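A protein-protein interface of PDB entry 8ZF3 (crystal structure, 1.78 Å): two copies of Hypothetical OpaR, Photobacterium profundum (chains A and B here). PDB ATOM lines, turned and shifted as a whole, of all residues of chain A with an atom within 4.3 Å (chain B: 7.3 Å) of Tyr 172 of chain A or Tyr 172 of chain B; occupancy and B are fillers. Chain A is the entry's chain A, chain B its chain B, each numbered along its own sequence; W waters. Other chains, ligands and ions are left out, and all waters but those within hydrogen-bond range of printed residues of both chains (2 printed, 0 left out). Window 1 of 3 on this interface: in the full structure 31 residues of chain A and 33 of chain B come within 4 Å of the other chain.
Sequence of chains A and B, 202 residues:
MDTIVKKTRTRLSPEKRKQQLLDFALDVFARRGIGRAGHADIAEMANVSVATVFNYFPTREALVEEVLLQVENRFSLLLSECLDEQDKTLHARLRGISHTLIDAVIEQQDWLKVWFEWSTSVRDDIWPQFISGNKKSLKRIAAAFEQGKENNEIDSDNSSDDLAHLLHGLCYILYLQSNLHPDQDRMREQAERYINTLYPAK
Water W1 lies within hydrogen-bond range of O of Thr 120 of chain B (2.6 Å) and OH of Tyr 175 of chain A (2.9 Å). Water W2 lies within hydrogen-bond range of OH of Tyr 175 of chain B (2.7 Å) and O of Thr 120 of chain A (2.7 Å).
Of the printed residues of chain A, Phe 116 of chain B touches Thr 120 (3.8 Å) and Tyr 172 (3.6 Å). Of the printed residues of chain A, Tyr 172 of chain B touches Phe 116 (3.7 Å), Ser 119 (2.7 Å), Thr 120 (3.995 Å) and Tyr 172 (3.5 Å). Of the printed residues of chain A, Leu 176 of chain B touches Ser 119. The nearest printed residue of chain B that does not touch Tyr 172 of chain A is Thr 120 of chain B (4.03 Å).
Along chain B the printed residues that touch a printed residue of chain A span positions 116 to 176. Of the 12 printed residues of chain A, 8 touch a printed residue of chain B. Hydrophobic or aromatic side chains of chain A that line the printed part of chain B: Phe 116, His 168, Tyr 172, Ile 173 and Leu 176. Among the printed residues, 19 pairs touch across the chains. Among the printed residues, no Asp or Glu carboxylate lies within 4 Å of a Lys or Arg side-chain nitrogen of the other chain.
NE2 of His 168 of chain B lies within hydrogen-bond range of OH of Tyr 172 of chain A (3.2 Å). The side-chain hydroxyl of Thr 120 of chain A is in hydrogen-bond range of the side-chain hydroxyl of Thr 120 of chain B (2.9 Å). The side-chain hydroxyl (OH) of Tyr 172 of chain A sits at hydrogen-bond distance from the side-chain hydroxyl (OG) of Ser 119 of chain B, 2.7 Å away. OH of Tyr 172 of chain B lies within hydrogen-bond range of OG of Ser 119 of chain A.
Ser 119 of chain A touches Leu 176 of chain B, and with the chains exchanged Leu 176 of chain A touches Ser 119 of chain B. Thr 120 of chain A touches its own counterpart, Thr 120 of chain B. His 168 of chain A touches Ile 173 of chain B, but with the chains exchanged Ile 173 of chain A does not touch His 168 of chain B (4.2 Å). Of the 19 pairs that touch across the chains among the printed residues, 13 have their exchanged pair printed and touching as well.
Among the printed residues, pairs that only touch across the chains: Ser 119 of chain A with Leu 176 of chain B (3.1 Å), Leu 176 of chain A with Ser 119 of chain B (3.3 Å), Ile 173 of chain A with His 165 of chain B (3.3 Å), Gly 169 of chain A with Ile 173 of chain B (3.3 Å), Ile 173 of chain A with Gly 169 of chain B (3.4 Å), Tyr 172 of chain A with Tyr 172 of chain B (3.5 Å), Ile 173 of chain A with Leu 166 of chain B (3.6 Å), His 168 of chain A with Ile 173 of chain B (3.6 Å), Leu 176 of chain A with His 168 of chain B (3.6 Å), Tyr 172 of chain A with Phe 116 of chain B (3.6 Å), Gly 169 of chain A with Gly 169 of chain B (3.7 Å), Phe 116 of chain A with Thr 120 of chain B (3.7 Å), Phe 116 of chain A with Tyr 172 of chain B (3.7 Å), Thr 120 of chain A with Phe 116 of chain B (3.8 Å) and Thr 120 of chain A with Tyr 172 of chain B (3.995 Å).
The backbone carbonyl oxygen (O) of Glu 117 of chain B sits at hydrogen-bond distance from the side-chain hydroxyl (OG1) of Thr 120 of chain B, 3.3 Å away. The side-chain hydroxyl (OG1) of Thr 120 of chain A lies within hydrogen-bond range of the backbone carbonyl oxygen (O) of Phe 116 of chain A (3.5 Å). O of Phe 116 of chain B lies within hydrogen-bond range of OG1 of Thr 120 of chain B (3.5 Å).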
ATOM      1  N   PHE A 116      19.039  -4.252  31.584  1.00  0.00           N
ATOM      2  CA  PHE A 116      20.492  -4.356  31.434  1.00  0.00           C
ATOM      3  C   PHE A 116      21.212  -4.428  32.774  1.00  0.00           C
ATOM      4  O   PHE A 116      22.236  -5.124  32.893  1.00  0.00           O
ATOM      5  CB  PHE A 116      21.021  -3.189  30.609  1.00  0.00           C
ATOM      6  CG  PHE A 116      20.959  -3.452  29.119  1.00  0.00           C
ATOM      7  CD1 PHE A 116      21.819  -4.366  28.534  1.00  0.00           C
ATOM      8  CD2 PHE A 116      20.006  -2.831  28.335  1.00  0.00           C
ATOM      9  CE1 PHE A 116      21.765  -4.647  27.157  1.00  0.00           C
ATOM     10  CE2 PHE A 116      19.928  -3.096  26.972  1.00  0.00           C
ATOM     11  CZ  PHE A 116      20.825  -4.004  26.376  1.00  0.00           C
ATOM     12  N   SER A 119      21.028  -7.903  33.849  1.00  0.00           N
ATOM     13  CA  SER A 119      21.898  -8.804  33.081  1.00  0.00           C
ATOM     14  C   SER A 119      23.312  -8.864  33.648  1.00  0.00           C
ATOM     15  O   SER A 119      23.964  -9.904  33.545  1.00  0.00           O
ATOM     16  CB  SER A 119      21.944  -8.380  31.606  1.00  0.00           C
ATOM     17  OG  SER A 119      22.851  -7.302  31.362  1.00  0.00           O
ATOM     18  N   THR A 120      23.812  -7.777  34.222  1.00  0.00           N
ATOM     19  CA  THR A 120      25.157  -7.763  34.787  1.00  0.00           C
ATOM     20  C   THR A 120      25.168  -8.037  36.286  1.00  0.00           C
ATOM     21  O   THR A 120      26.220  -7.912  36.916  1.00  0.00           O
ATOM     22  CB  THR A 120      25.844  -6.423  34.488  1.00  0.00           C
ATOM     23  OG1 THR A 120      25.021  -5.351  34.966  1.00  0.00           O
ATOM     24  CG2 THR A 120      25.999  -6.244  32.983  1.00  0.00           C
ATOM     25  N   HIS A 168      22.283  -9.920  21.028  1.00  0.00           N
ATOM     26  CA  HIS A 168      22.248  -9.316  22.355  1.00  0.00           C
ATOM     27  C   HIS A 168      23.464  -8.431  22.570  1.00  0.00           C
ATOM     28  O   HIS A 168      23.358  -7.357  23.177  1.00  0.00           O
ATOM     29  CB  HIS A 168      22.164 -10.388  23.443  1.00  0.00           C
ATOM     30  CG  HIS A 168      20.771 -10.856  23.713  1.00  0.00           C
ATOM     31  ND1 HIS A 168      19.674 -10.028  23.610  1.00  0.00           N
ATOM     32  CD2 HIS A 168      20.297 -12.058  24.111  1.00  0.00           C
ATOM     33  CE1 HIS A 168      18.581 -10.706  23.910  1.00  0.00           C
ATOM     34  NE2 HIS A 168      18.932 -11.939  24.219  1.00  0.00           N
ATOM     35  N   GLY A 169      24.628  -8.854  22.064  1.00  0.00           N
ATOM     36  CA  GLY A 169      25.808  -8.001  22.151  1.00  0.00           C
ATOM     37  C   GLY A 169      25.643  -6.697  21.381  1.00  0.00           C
ATOM     38  O   GLY A 169      26.074  -5.626  21.833  1.00  0.00           O
ATOM     39  N   LEU A 170      25.028  -6.768  20.205  1.00  0.00           N
ATOM     40  CA  LEU A 170      24.704  -5.548  19.474  1.00  0.00           C
ATOM     41  C   LEU A 170      23.772  -4.653  20.285  1.00  0.00           C
ATOM     42  O   LEU A 170      23.984  -3.437  20.380  1.00  0.00           O
ATOM     43  CB  LEU A 170      24.087  -5.915  18.117  1.00  0.00           C
ATOM     44  CG  LEU A 170      23.323  -4.852  17.309  1.00  0.00           C
ATOM     45  CD1 LEU A 170      24.161  -3.643  17.208  1.00  0.00           C
ATOM     46  CD2 LEU A 170      23.050  -5.387  15.892  1.00  0.00           C
ATOM     47  N   CYS A 171      22.741  -5.240  20.894  1.00  0.00           N
ATOM     48  CA  CYS A 171      21.788  -4.445  21.653  1.00  0.00           C
ATOM     49  C   CYS A 171      22.495  -3.753  22.813  1.00  0.00           C
ATOM     50  O   CYS A 171      22.230  -2.582  23.111  1.00  0.00           O
ATOM     51  CB  CYS A 171      20.668  -5.351  22.152  1.00  0.00           C
ATOM     52  SG  CYS A 171      19.462  -5.771  20.831  1.00  0.00           S
ATOM     53  N   TYR A 172      23.452  -4.450  23.428  1.00  0.00           N
ATOM     54  CA  TYR A 172      24.200  -3.883  24.547  1.00  0.00           C
ATOM     55  C   TYR A 172      24.968  -2.640  24.116  1.00  0.00           C
ATOM     56  O   TYR A 172      24.874  -1.583  24.763  1.00  0.00           O
ATOM     57  CB  TYR A 172      25.145  -4.950  25.118  1.00  0.00           C
ATOM     58  CG  TYR A 172      26.168  -4.495  26.137  1.00  0.00           C
ATOM     59  CD1 TYR A 172      25.782  -4.156  27.438  1.00  0.00           C
ATOM     60  CD2 TYR A 172      27.515  -4.406  25.810  1.00  0.00           C
ATOM     61  CE1 TYR A 172      26.738  -3.766  28.391  1.00  0.00           C
ATOM     62  CE2 TYR A 172      28.480  -4.013  26.767  1.00  0.00           C
ATOM     63  CZ  TYR A 172      28.079  -3.691  28.039  1.00  0.00           C
ATOM     64  OH  TYR A 172      29.043  -3.325  28.954  1.00  0.00           O
ATOM     65  N   ILE A 173      25.712  -2.724  23.003  1.00  0.00           N
ATOM     66  CA  ILE A 173      26.521  -1.572  22.612  1.00  0.00           C
ATOM     67  C   ILE A 173      25.623  -0.448  22.105  1.00  0.00           C
ATOM     68  O   ILE A 173      25.896   0.730  22.353  1.00  0.00           O
ATOM     69  CB  ILE A 173      27.596  -1.941  21.571  1.00  0.00           C
ATOM     70  CG1 ILE A 173      26.949  -2.430  20.272  1.00  0.00           C
ATOM     71  CG2 ILE A 173      28.595  -2.950  22.191  1.00  0.00           C
ATOM     72  CD1 ILE A 173      27.887  -3.134  19.294  1.00  0.00           C
ATOM     73  N   LEU A 174      24.545  -0.797  21.398  1.00  0.00           N
ATOM     74  CA  LEU A 174      23.571   0.200  20.976  1.00  0.00           C
ATOM     75  C   LEU A 174      22.930   0.854  22.190  1.00  0.00           C
ATOM     76  O   LEU A 174      22.655   2.056  22.177  1.00  0.00           O
ATOM     77  CB  LEU A 174      22.511  -0.470  20.081  1.00  0.00           C
ATOM     78  CG  LEU A 174      22.352  -0.182  18.581  1.00  0.00           C
ATOM     79  CD1 LEU A 174      20.978  -0.683  18.133  1.00  0.00           C
ATOM     80  CD2 LEU A 174      22.552   1.304  18.205  1.00  0.00           C
ATOM     81  N   TYR A 175      22.742   0.085  23.266  1.00  0.00           N
ATOM     82  CA  TYR A 175      22.151   0.622  24.481  1.00  0.00           C
ATOM     83  C   TYR A 175      23.075   1.659  25.111  1.00  0.00           C
ATOM     84  O   TYR A 175      22.648   2.776  25.435  1.00  0.00           O
ATOM     85  CB  TYR A 175      21.874  -0.525  25.450  1.00  0.00           C
ATOM     86  CG  TYR A 175      21.427  -0.061  26.802  1.00  0.00           C
ATOM     87  CD1 TYR A 175      20.125   0.381  27.003  1.00  0.00           C
ATOM     88  CD2 TYR A 175      22.306  -0.043  27.871  1.00  0.00           C
ATOM     89  CE1 TYR A 175      19.698   0.798  28.235  1.00  0.00           C
ATOM     90  CE2 TYR A 175      21.891   0.395  29.134  1.00  0.00           C
ATOM     91  CZ  TYR A 175      20.587   0.807  29.305  1.00  0.00           C
ATOM     92  OH  TYR A 175      20.160   1.249  30.535  1.00  0.00           O
ATOM     93  N   LEU A 176      24.359   1.311  25.259  1.00  0.00           N
ATOM     94  CA  LEU A 176      25.326   2.253  25.820  1.00  0.00           C
ATOM     95  C   LEU A 176      25.476   3.482  24.939  1.00  0.00           C
ATOM     96  O   LEU A 176      25.513   4.615  25.436  1.00  0.00           O
ATOM     97  CB  LEU A 176      26.687   1.590  25.992  1.00  0.00           C
ATOM     98  CG  LEU A 176      26.710   0.329  26.847  1.00  0.00           C
ATOM     99  CD1 LEU A 176      28.166  -0.140  26.952  1.00  0.00           C
ATOM    100  CD2 LEU A 176      26.084   0.605  28.198  1.00  0.00           C
ATOM    101  N   LEU B 101      39.604 -12.589  29.287  1.00  0.00           N
ATOM    102  CA  LEU B 101      38.281 -12.332  29.854  1.00  0.00           C
ATOM    103  C   LEU B 101      37.655 -13.595  30.431  1.00  0.00           C
ATOM    104  O   LEU B 101      37.106 -13.571  31.539  1.00  0.00           O
ATOM    105  CB  LEU B 101      37.370 -11.711  28.793  1.00  0.00           C
ATOM    106  CG  LEU B 101      35.968 -11.244  29.206  1.00  0.00           C
ATOM    107  CD1 LEU B 101      35.491 -10.347  28.118  1.00  0.00           C
ATOM    108  CD2 LEU B 101      34.934 -12.385  29.350  1.00  0.00           C
ATOM    109  N   TRP B 115      33.482  -3.742  36.681  1.00  0.00           N
ATOM    110  CA  TRP B 115      33.550  -3.032  35.411  1.00  0.00           C
ATOM    111  C   TRP B 115      32.235  -3.167  34.645  1.00  0.00           C
ATOM    112  O   TRP B 115      31.675  -2.176  34.155  1.00  0.00           O
ATOM    113  CB  TRP B 115      34.721  -3.571  34.578  1.00  0.00           C
ATOM    114  CG  TRP B 115      35.079  -2.697  33.393  1.00  0.00           C
ATOM    115  CD1 TRP B 115      35.898  -1.591  33.380  1.00  0.00           C
ATOM    116  CD2 TRP B 115      34.577  -2.835  32.062  1.00  0.00           C
ATOM    117  NE1 TRP B 115      35.965  -1.062  32.105  1.00  0.00           N
ATOM    118  CE2 TRP B 115      35.160  -1.808  31.281  1.00  0.00           C
ATOM    119  CE3 TRP B 115      33.703  -3.738  31.454  1.00  0.00           C
ATOM    120  CZ2 TRP B 115      34.885  -1.657  29.923  1.00  0.00           C
ATOM    121  CZ3 TRP B 115      33.423  -3.583  30.102  1.00  0.00           C
ATOM    122  CH2 TRP B 115      34.013  -2.549  29.355  1.00  0.00           C
ATOM    123  N   PHE B 116      31.718  -4.397  34.541  1.00  0.00           N
ATOM    124  CA  PHE B 116      30.464  -4.574  33.816  1.00  0.00           C
ATOM    125  C   PHE B 116      29.269  -3.972  34.557  1.00  0.00           C
ATOM    126  O   PHE B 116      28.351  -3.443  33.909  1.00  0.00           O
ATOM    127  CB  PHE B 116      30.241  -6.052  33.506  1.00  0.00           C
ATOM    128  CG  PHE B 116      30.838  -6.475  32.192  1.00  0.00           C
ATOM    129  CD1 PHE B 116      30.250  -6.070  31.010  1.00  0.00           C
ATOM    130  CD2 PHE B 116      31.995  -7.259  32.136  1.00  0.00           C
ATOM    131  CE1 PHE B 116      30.795  -6.457  29.768  1.00  0.00           C
ATOM    132  CE2 PHE B 116      32.549  -7.639  30.904  1.00  0.00           C
ATOM    133  CZ  PHE B 116      31.930  -7.239  29.722  1.00  0.00           C
ATOM    134  N   GLU B 117      29.257  -3.998  35.904  1.00  0.00           N
ATOM    135  CA  GLU B 117      28.172  -3.308  36.604  1.00  0.00           C
ATOM    136  C   GLU B 117      28.257  -1.805  36.352  1.00  0.00           C
ATOM    137  O   GLU B 117      27.231  -1.134  36.143  1.00  0.00           O
ATOM    138  CB  GLU B 117      28.189  -3.564  38.130  1.00  0.00           C
ATOM    139  CG  GLU B 117      27.264  -2.538  38.805  1.00  0.00           C
ATOM    140  CD  GLU B 117      27.114  -2.599  40.338  1.00  0.00           C
ATOM    141  OE1 GLU B 117      27.871  -3.314  41.028  1.00  0.00           O
ATOM    142  OE2 GLU B 117      26.205  -1.906  40.845  1.00  0.00           O
ATOM    143  N   TRP B 118      29.477  -1.260  36.367  1.00  0.00           N
ATOM    144  CA  TRP B 118      29.686   0.151  36.054  1.00  0.00           C
ATOM    145  C   TRP B 118      29.101   0.497  34.694  1.00  0.00           C
ATOM    146  O   TRP B 118      28.488   1.558  34.513  1.00  0.00           O
ATOM    147  CB  TRP B 118      31.178   0.426  36.067  1.00  0.00           C
ATOM    148  CG  TRP B 118      31.634   1.819  36.050  1.00  0.00           C
ATOM    149  CD1 TRP B 118      30.896   2.958  36.242  1.00  0.00           C
ATOM    150  CD2 TRP B 118      32.993   2.231  35.911  1.00  0.00           C
ATOM    151  NE1 TRP B 118      31.725   4.057  36.208  1.00  0.00           N
ATOM    152  CE2 TRP B 118      33.016   3.634  35.998  1.00  0.00           C
ATOM    153  CE3 TRP B 118      34.193   1.538  35.705  1.00  0.00           C
ATOM    154  CZ2 TRP B 118      34.201   4.370  35.878  1.00  0.00           C
ATOM    155  CZ3 TRP B 118      35.370   2.266  35.592  1.00  0.00           C
ATOM    156  CH2 TRP B 118      35.365   3.662  35.680  1.00  0.00           C
ATOM    157  N   SER B 119      29.287  -0.401  33.727  1.00  0.00           N
ATOM    158  CA  SER B 119      28.928  -0.122  32.342  1.00  0.00           C
ATOM    159  C   SER B 119      27.430   0.081  32.183  1.00  0.00           C
ATOM    160  O   SER B 119      26.999   0.856  31.319  1.00  0.00           O
ATOM    161  CB  SER B 119      29.421  -1.262  31.431  1.00  0.00           C
ATOM    162  OG  SER B 119      28.531  -2.381  31.408  1.00  0.00           O
ATOM    163  N   THR B 120      26.619  -0.608  32.984  1.00  0.00           N
ATOM    164  CA  THR B 120      25.171  -0.491  32.873  1.00  0.00           C
ATOM    165  C   THR B 120      24.598   0.487  33.902  1.00  0.00           C
ATOM    166  O   THR B 120      23.373   0.570  34.052  1.00  0.00           O
ATOM    167  CB  THR B 120      24.511  -1.871  33.010  1.00  0.00           C
ATOM    168  OG1 THR B 120      24.990  -2.524  34.193  1.00  0.00           O
ATOM    169  CG2 THR B 120      24.855  -2.770  31.810  1.00  0.00           C
ATOM    170  N   PHE B 130      32.886   6.147  33.322  1.00  0.00           N
ATOM    171  CA  PHE B 130      32.978   4.899  32.572  1.00  0.00           C
ATOM    172  C   PHE B 130      33.273   5.193  31.107  1.00  0.00           C
ATOM    173  O   PHE B 130      34.169   4.587  30.500  1.00  0.00           O
ATOM    174  CB  PHE B 130      31.704   4.051  32.704  1.00  0.00           C
ATOM    175  CG  PHE B 130      31.715   2.844  31.807  1.00  0.00           C
ATOM    176  CD1 PHE B 130      32.409   1.704  32.183  1.00  0.00           C
ATOM    177  CD2 PHE B 130      31.055   2.845  30.578  1.00  0.00           C
ATOM    178  CE1 PHE B 130      32.475   0.588  31.364  1.00  0.00           C
ATOM    179  CE2 PHE B 130      31.099   1.733  29.752  1.00  0.00           C
ATOM    180  CZ  PHE B 130      31.819   0.591  30.135  1.00  0.00           C
ATOM    181  N   HIS B 165      33.738  -1.132  18.831  1.00  0.00           N
ATOM    182  CA  HIS B 165      32.505  -1.203  19.602  1.00  0.00           C
ATOM    183  C   HIS B 165      31.936  -2.613  19.613  1.00  0.00           C
ATOM    184  O   HIS B 165      31.548  -3.122  20.668  1.00  0.00           O
ATOM    185  CB  HIS B 165      31.523  -0.188  19.035  1.00  0.00           C
ATOM    186  CG  HIS B 165      31.842   1.220  19.426  1.00  0.00           C
ATOM    187  ND1 HIS B 165      31.991   2.236  18.511  1.00  0.00           N
ATOM    188  CD2 HIS B 165      31.966   1.794  20.648  1.00  0.00           C
ATOM    189  CE1 HIS B 165      32.238   3.369  19.144  1.00  0.00           C
ATOM    190  NE2 HIS B 165      32.221   3.131  20.444  1.00  0.00           N
ATOM    191  N   LEU B 166      31.926  -3.277  18.456  1.00  0.00           N
ATOM    192  CA  LEU B 166      31.389  -4.633  18.377  1.00  0.00           C
ATOM    193  C   LEU B 166      32.183  -5.601  19.236  1.00  0.00           C
ATOM    194  O   LEU B 166      31.617  -6.561  19.776  1.00  0.00           O
ATOM    195  CB  LEU B 166      31.374  -5.107  16.935  1.00  0.00           C
ATOM    196  CG  LEU B 166      30.260  -4.488  16.085  1.00  0.00           C
ATOM    197  CD1 LEU B 166      30.587  -4.750  14.642  1.00  0.00           C
ATOM    198  CD2 LEU B 166      28.920  -5.081  16.458  1.00  0.00           C
ATOM    199  N   LEU B 167      33.481  -5.357  19.400  1.00  0.00           N
ATOM    200  CA  LEU B 167      34.271  -6.215  20.277  1.00  0.00           C
ATOM    201  C   LEU B 167      33.786  -6.124  21.719  1.00  0.00           C
ATOM    202  O   LEU B 167      33.766  -7.130  22.446  1.00  0.00           O
ATOM    203  CB  LEU B 167      35.739  -5.831  20.199  1.00  0.00           C
ATOM    204  CG  LEU B 167      36.616  -6.740  21.087  1.00  0.00           C
ATOM    205  CD1 LEU B 167      36.456  -8.199  20.690  1.00  0.00           C
ATOM    206  CD2 LEU B 167      38.039  -6.294  20.928  1.00  0.00           C
ATOM    207  N   HIS B 168      33.421  -4.917  22.158  1.00  0.00           N
ATOM    208  CA  HIS B 168      32.843  -4.752  23.480  1.00  0.00           C
ATOM    209  C   HIS B 168      31.582  -5.590  23.632  1.00  0.00           C
ATOM    210  O   HIS B 168      31.373  -6.230  24.669  1.00  0.00           O
ATOM    211  CB  HIS B 168      32.550  -3.272  23.719  1.00  0.00           C
ATOM    212  CG  HIS B 168      32.154  -2.951  25.123  1.00  0.00           C
ATOM    213  ND1 HIS B 168      31.681  -1.712  25.491  1.00  0.00           N
ATOM    214  CD2 HIS B 168      32.176  -3.698  26.250  1.00  0.00           C
ATOM    215  CE1 HIS B 168      31.425  -1.709  26.787  1.00  0.00           C
ATOM    216  NE2 HIS B 168      31.709  -2.904  27.270  1.00  0.00           N
ATOM    217  N   GLY B 169      30.728  -5.599  22.604  1.00  0.00           N
ATOM    218  CA  GLY B 169      29.539  -6.442  22.647  1.00  0.00           C
ATOM    219  C   GLY B 169      29.886  -7.918  22.711  1.00  0.00           C
ATOM    220  O   GLY B 169      29.212  -8.700  23.388  1.00  0.00           O
ATOM    221  N   LEU B 170      30.938  -8.325  21.990  1.00  0.00           N
ATOM    222  CA  LEU B 170      31.346  -9.720  22.066  1.00  0.00           C
ATOM    223  C   LEU B 170      31.816 -10.059  23.471  1.00  0.00           C
ATOM    224  O   LEU B 170      31.468 -11.125  23.994  1.00  0.00           O
ATOM    225  CB  LEU B 170      32.441 -10.011  21.040  1.00  0.00           C
ATOM    226  CG  LEU B 170      32.813 -11.485  20.825  1.00  0.00           C
ATOM    227  CD1 LEU B 170      33.373 -11.609  19.409  1.00  0.00           C
ATOM    228  CD2 LEU B 170      33.814 -11.997  21.818  1.00  0.00           C
ATOM    229  N   CYS B 171      32.607  -9.160  24.094  1.00  0.00           N
ATOM    230  CA  CYS B 171      33.052  -9.351  25.472  1.00  0.00           C
ATOM    231  C   CYS B 171      31.894  -9.445  26.456  1.00  0.00           C
ATOM    232  O   CYS B 171      31.936 -10.258  27.383  1.00  0.00           O
ATOM    233  CB  CYS B 171      34.043  -8.264  25.903  1.00  0.00           C
ATOM    234  SG  CYS B 171      35.645  -8.283  24.995  1.00  0.00           S
ATOM    235  N   TYR B 172      30.855  -8.639  26.262  1.00  0.00           N
ATOM    236  CA  TYR B 172      29.690  -8.696  27.134  1.00  0.00           C
ATOM    237  C   TYR B 172      29.039 -10.070  27.071  1.00  0.00           C
ATOM    238  O   TYR B 172      28.739 -10.681  28.106  1.00  0.00           O
ATOM    239  CB  TYR B 172      28.723  -7.579  26.723  1.00  0.00           C
ATOM    240  CG  TYR B 172      27.325  -7.632  27.293  1.00  0.00           C
ATOM    241  CD1 TYR B 172      27.074  -7.223  28.600  1.00  0.00           C
ATOM    242  CD2 TYR B 172      26.251  -8.046  26.508  1.00  0.00           C
ATOM    243  CE1 TYR B 172      25.787  -7.238  29.119  1.00  0.00           C
ATOM    244  CE2 TYR B 172      24.966  -8.086  27.008  1.00  0.00           C
ATOM    245  CZ  TYR B 172      24.732  -7.660  28.307  1.00  0.00           C
ATOM    246  OH  TYR B 172      23.473  -7.690  28.795  1.00  0.00           O
ATOM    247  N   ILE B 173      28.815 -10.584  25.853  1.00  0.00           N
ATOM    248  CA  ILE B 173      28.161 -11.874  25.713  1.00  0.00           C
ATOM    249  C   ILE B 173      29.034 -12.984  26.287  1.00  0.00           C
ATOM    250  O   ILE B 173      28.541 -13.889  26.969  1.00  0.00           O
ATOM    251  CB  ILE B 173      27.814 -12.140  24.237  1.00  0.00           C
ATOM    252  CG1 ILE B 173      26.848 -11.070  23.708  1.00  0.00           C
ATOM    253  CG2 ILE B 173      27.218 -13.524  24.083  1.00  0.00           C
ATOM    254  CD1 ILE B 173      25.565 -10.925  24.495  1.00  0.00           C
ATOM    255  N   LEU B 174      30.339 -12.932  26.009  1.00  0.00           N
ATOM    256  CA  LEU B 174      31.259 -13.928  26.557  1.00  0.00           C
ATOM    257  C   LEU B 174      31.272 -13.859  28.071  1.00  0.00           C
ATOM    258  O   LEU B 174      31.381 -14.880  28.757  1.00  0.00           O
ATOM    259  CB  LEU B 174      32.672 -13.674  26.046  1.00  0.00           C
ATOM    260  CG  LEU B 174      33.212 -14.387  24.807  1.00  0.00           C
ATOM    261  CD1 LEU B 174      34.671 -13.956  24.655  1.00  0.00           C
ATOM    262  CD2 LEU B 174      33.029 -15.911  24.760  1.00  0.00           C
ATOM    263  N   TYR B 175      31.190 -12.639  28.607  1.00  0.00           N
ATOM    264  CA  TYR B 175      31.184 -12.452  30.050  1.00  0.00           C
ATOM    265  C   TYR B 175      29.967 -13.123  30.692  1.00  0.00           C
ATOM    266  O   TYR B 175      30.089 -13.845  31.692  1.00  0.00           O
ATOM    267  CB  TYR B 175      31.223 -10.951  30.343  1.00  0.00           C
ATOM    268  CG  TYR B 175      31.031 -10.619  31.776  1.00  0.00           C
ATOM    269  CD1 TYR B 175      32.075 -10.796  32.678  1.00  0.00           C
ATOM    270  CD2 TYR B 175      29.813 -10.158  32.255  1.00  0.00           C
ATOM    271  CE1 TYR B 175      31.921 -10.498  34.003  1.00  0.00           C
ATOM    272  CE2 TYR B 175      29.647  -9.861  33.605  1.00  0.00           C
ATOM    273  CZ  TYR B 175      30.708 -10.043  34.467  1.00  0.00           C
ATOM    274  OH  TYR B 175      30.575  -9.760  35.813  1.00  0.00           O
ATOM    275  N   LEU B 176      28.772 -12.872  30.147  1.00  0.00           N
ATOM    276  CA  LEU B 176      27.568 -13.496  30.678  1.00  0.00           C
ATOM    277  C   LEU B 176      27.608 -15.012  30.520  1.00  0.00           C
ATOM    278  O   LEU B 176      27.212 -15.750  31.429  1.00  0.00           O
ATOM    279  CB  LEU B 176      26.319 -12.925  29.988  1.00  0.00           C
ATOM    280  CG  LEU B 176      26.115 -11.419  30.097  1.00  0.00           C
ATOM    281  CD1 LEU B 176      24.790 -11.014  29.418  1.00  0.00           C
ATOM    282  CD2 LEU B 176      26.139 -11.002  31.551  1.00  0.00           C
ATOM    283  N   GLN B 177      28.040 -15.497  29.358  1.00  0.00           N
ATOM    284  CA  GLN B 177      27.986 -16.938  29.141  1.00  0.00           C
ATOM    285  C   GLN B 177      29.000 -17.662  30.013  1.00  0.00           C
ATOM    286  O   GLN B 177      28.735 -18.775  30.472  1.00  0.00           O
ATOM    287  CB  GLN B 177      28.234 -17.268  27.673  1.00  0.00           C
ATOM    288  CG  GLN B 177      27.176 -16.786  26.726  1.00  0.00           C
ATOM    289  CD  GLN B 177      27.495 -17.226  25.319  1.00  0.00           C
ATOM    290  OE1 GLN B 177      28.306 -16.597  24.638  1.00  0.00           O
ATOM    291  NE2 GLN B 177      26.872 -18.307  24.876  1.00  0.00           N
ATOM    292  N   SER B 178      30.173 -17.051  30.220  1.00  0.00           N
ATOM    293  CA  SER B 178      31.204 -17.633  31.083  1.00  0.00           C
ATOM    294  C   SER B 178      30.755 -17.666  32.541  1.00  0.00           C
ATOM    295  O   SER B 178      31.172 -18.548  33.307  1.00  0.00           O
ATOM    296  CB  SER B 178      32.491 -16.823  30.968  1.00  0.00           C
ATOM    297  OG  SER B 178      33.088 -16.985  29.688  1.00  0.00           O
HETATM  298  O   HOH W   1      21.270  -0.183  32.736  1.00  0.00           O
HETATM  299  O   HOH W   2      28.884  -7.787  36.491  1.00  0.00           O
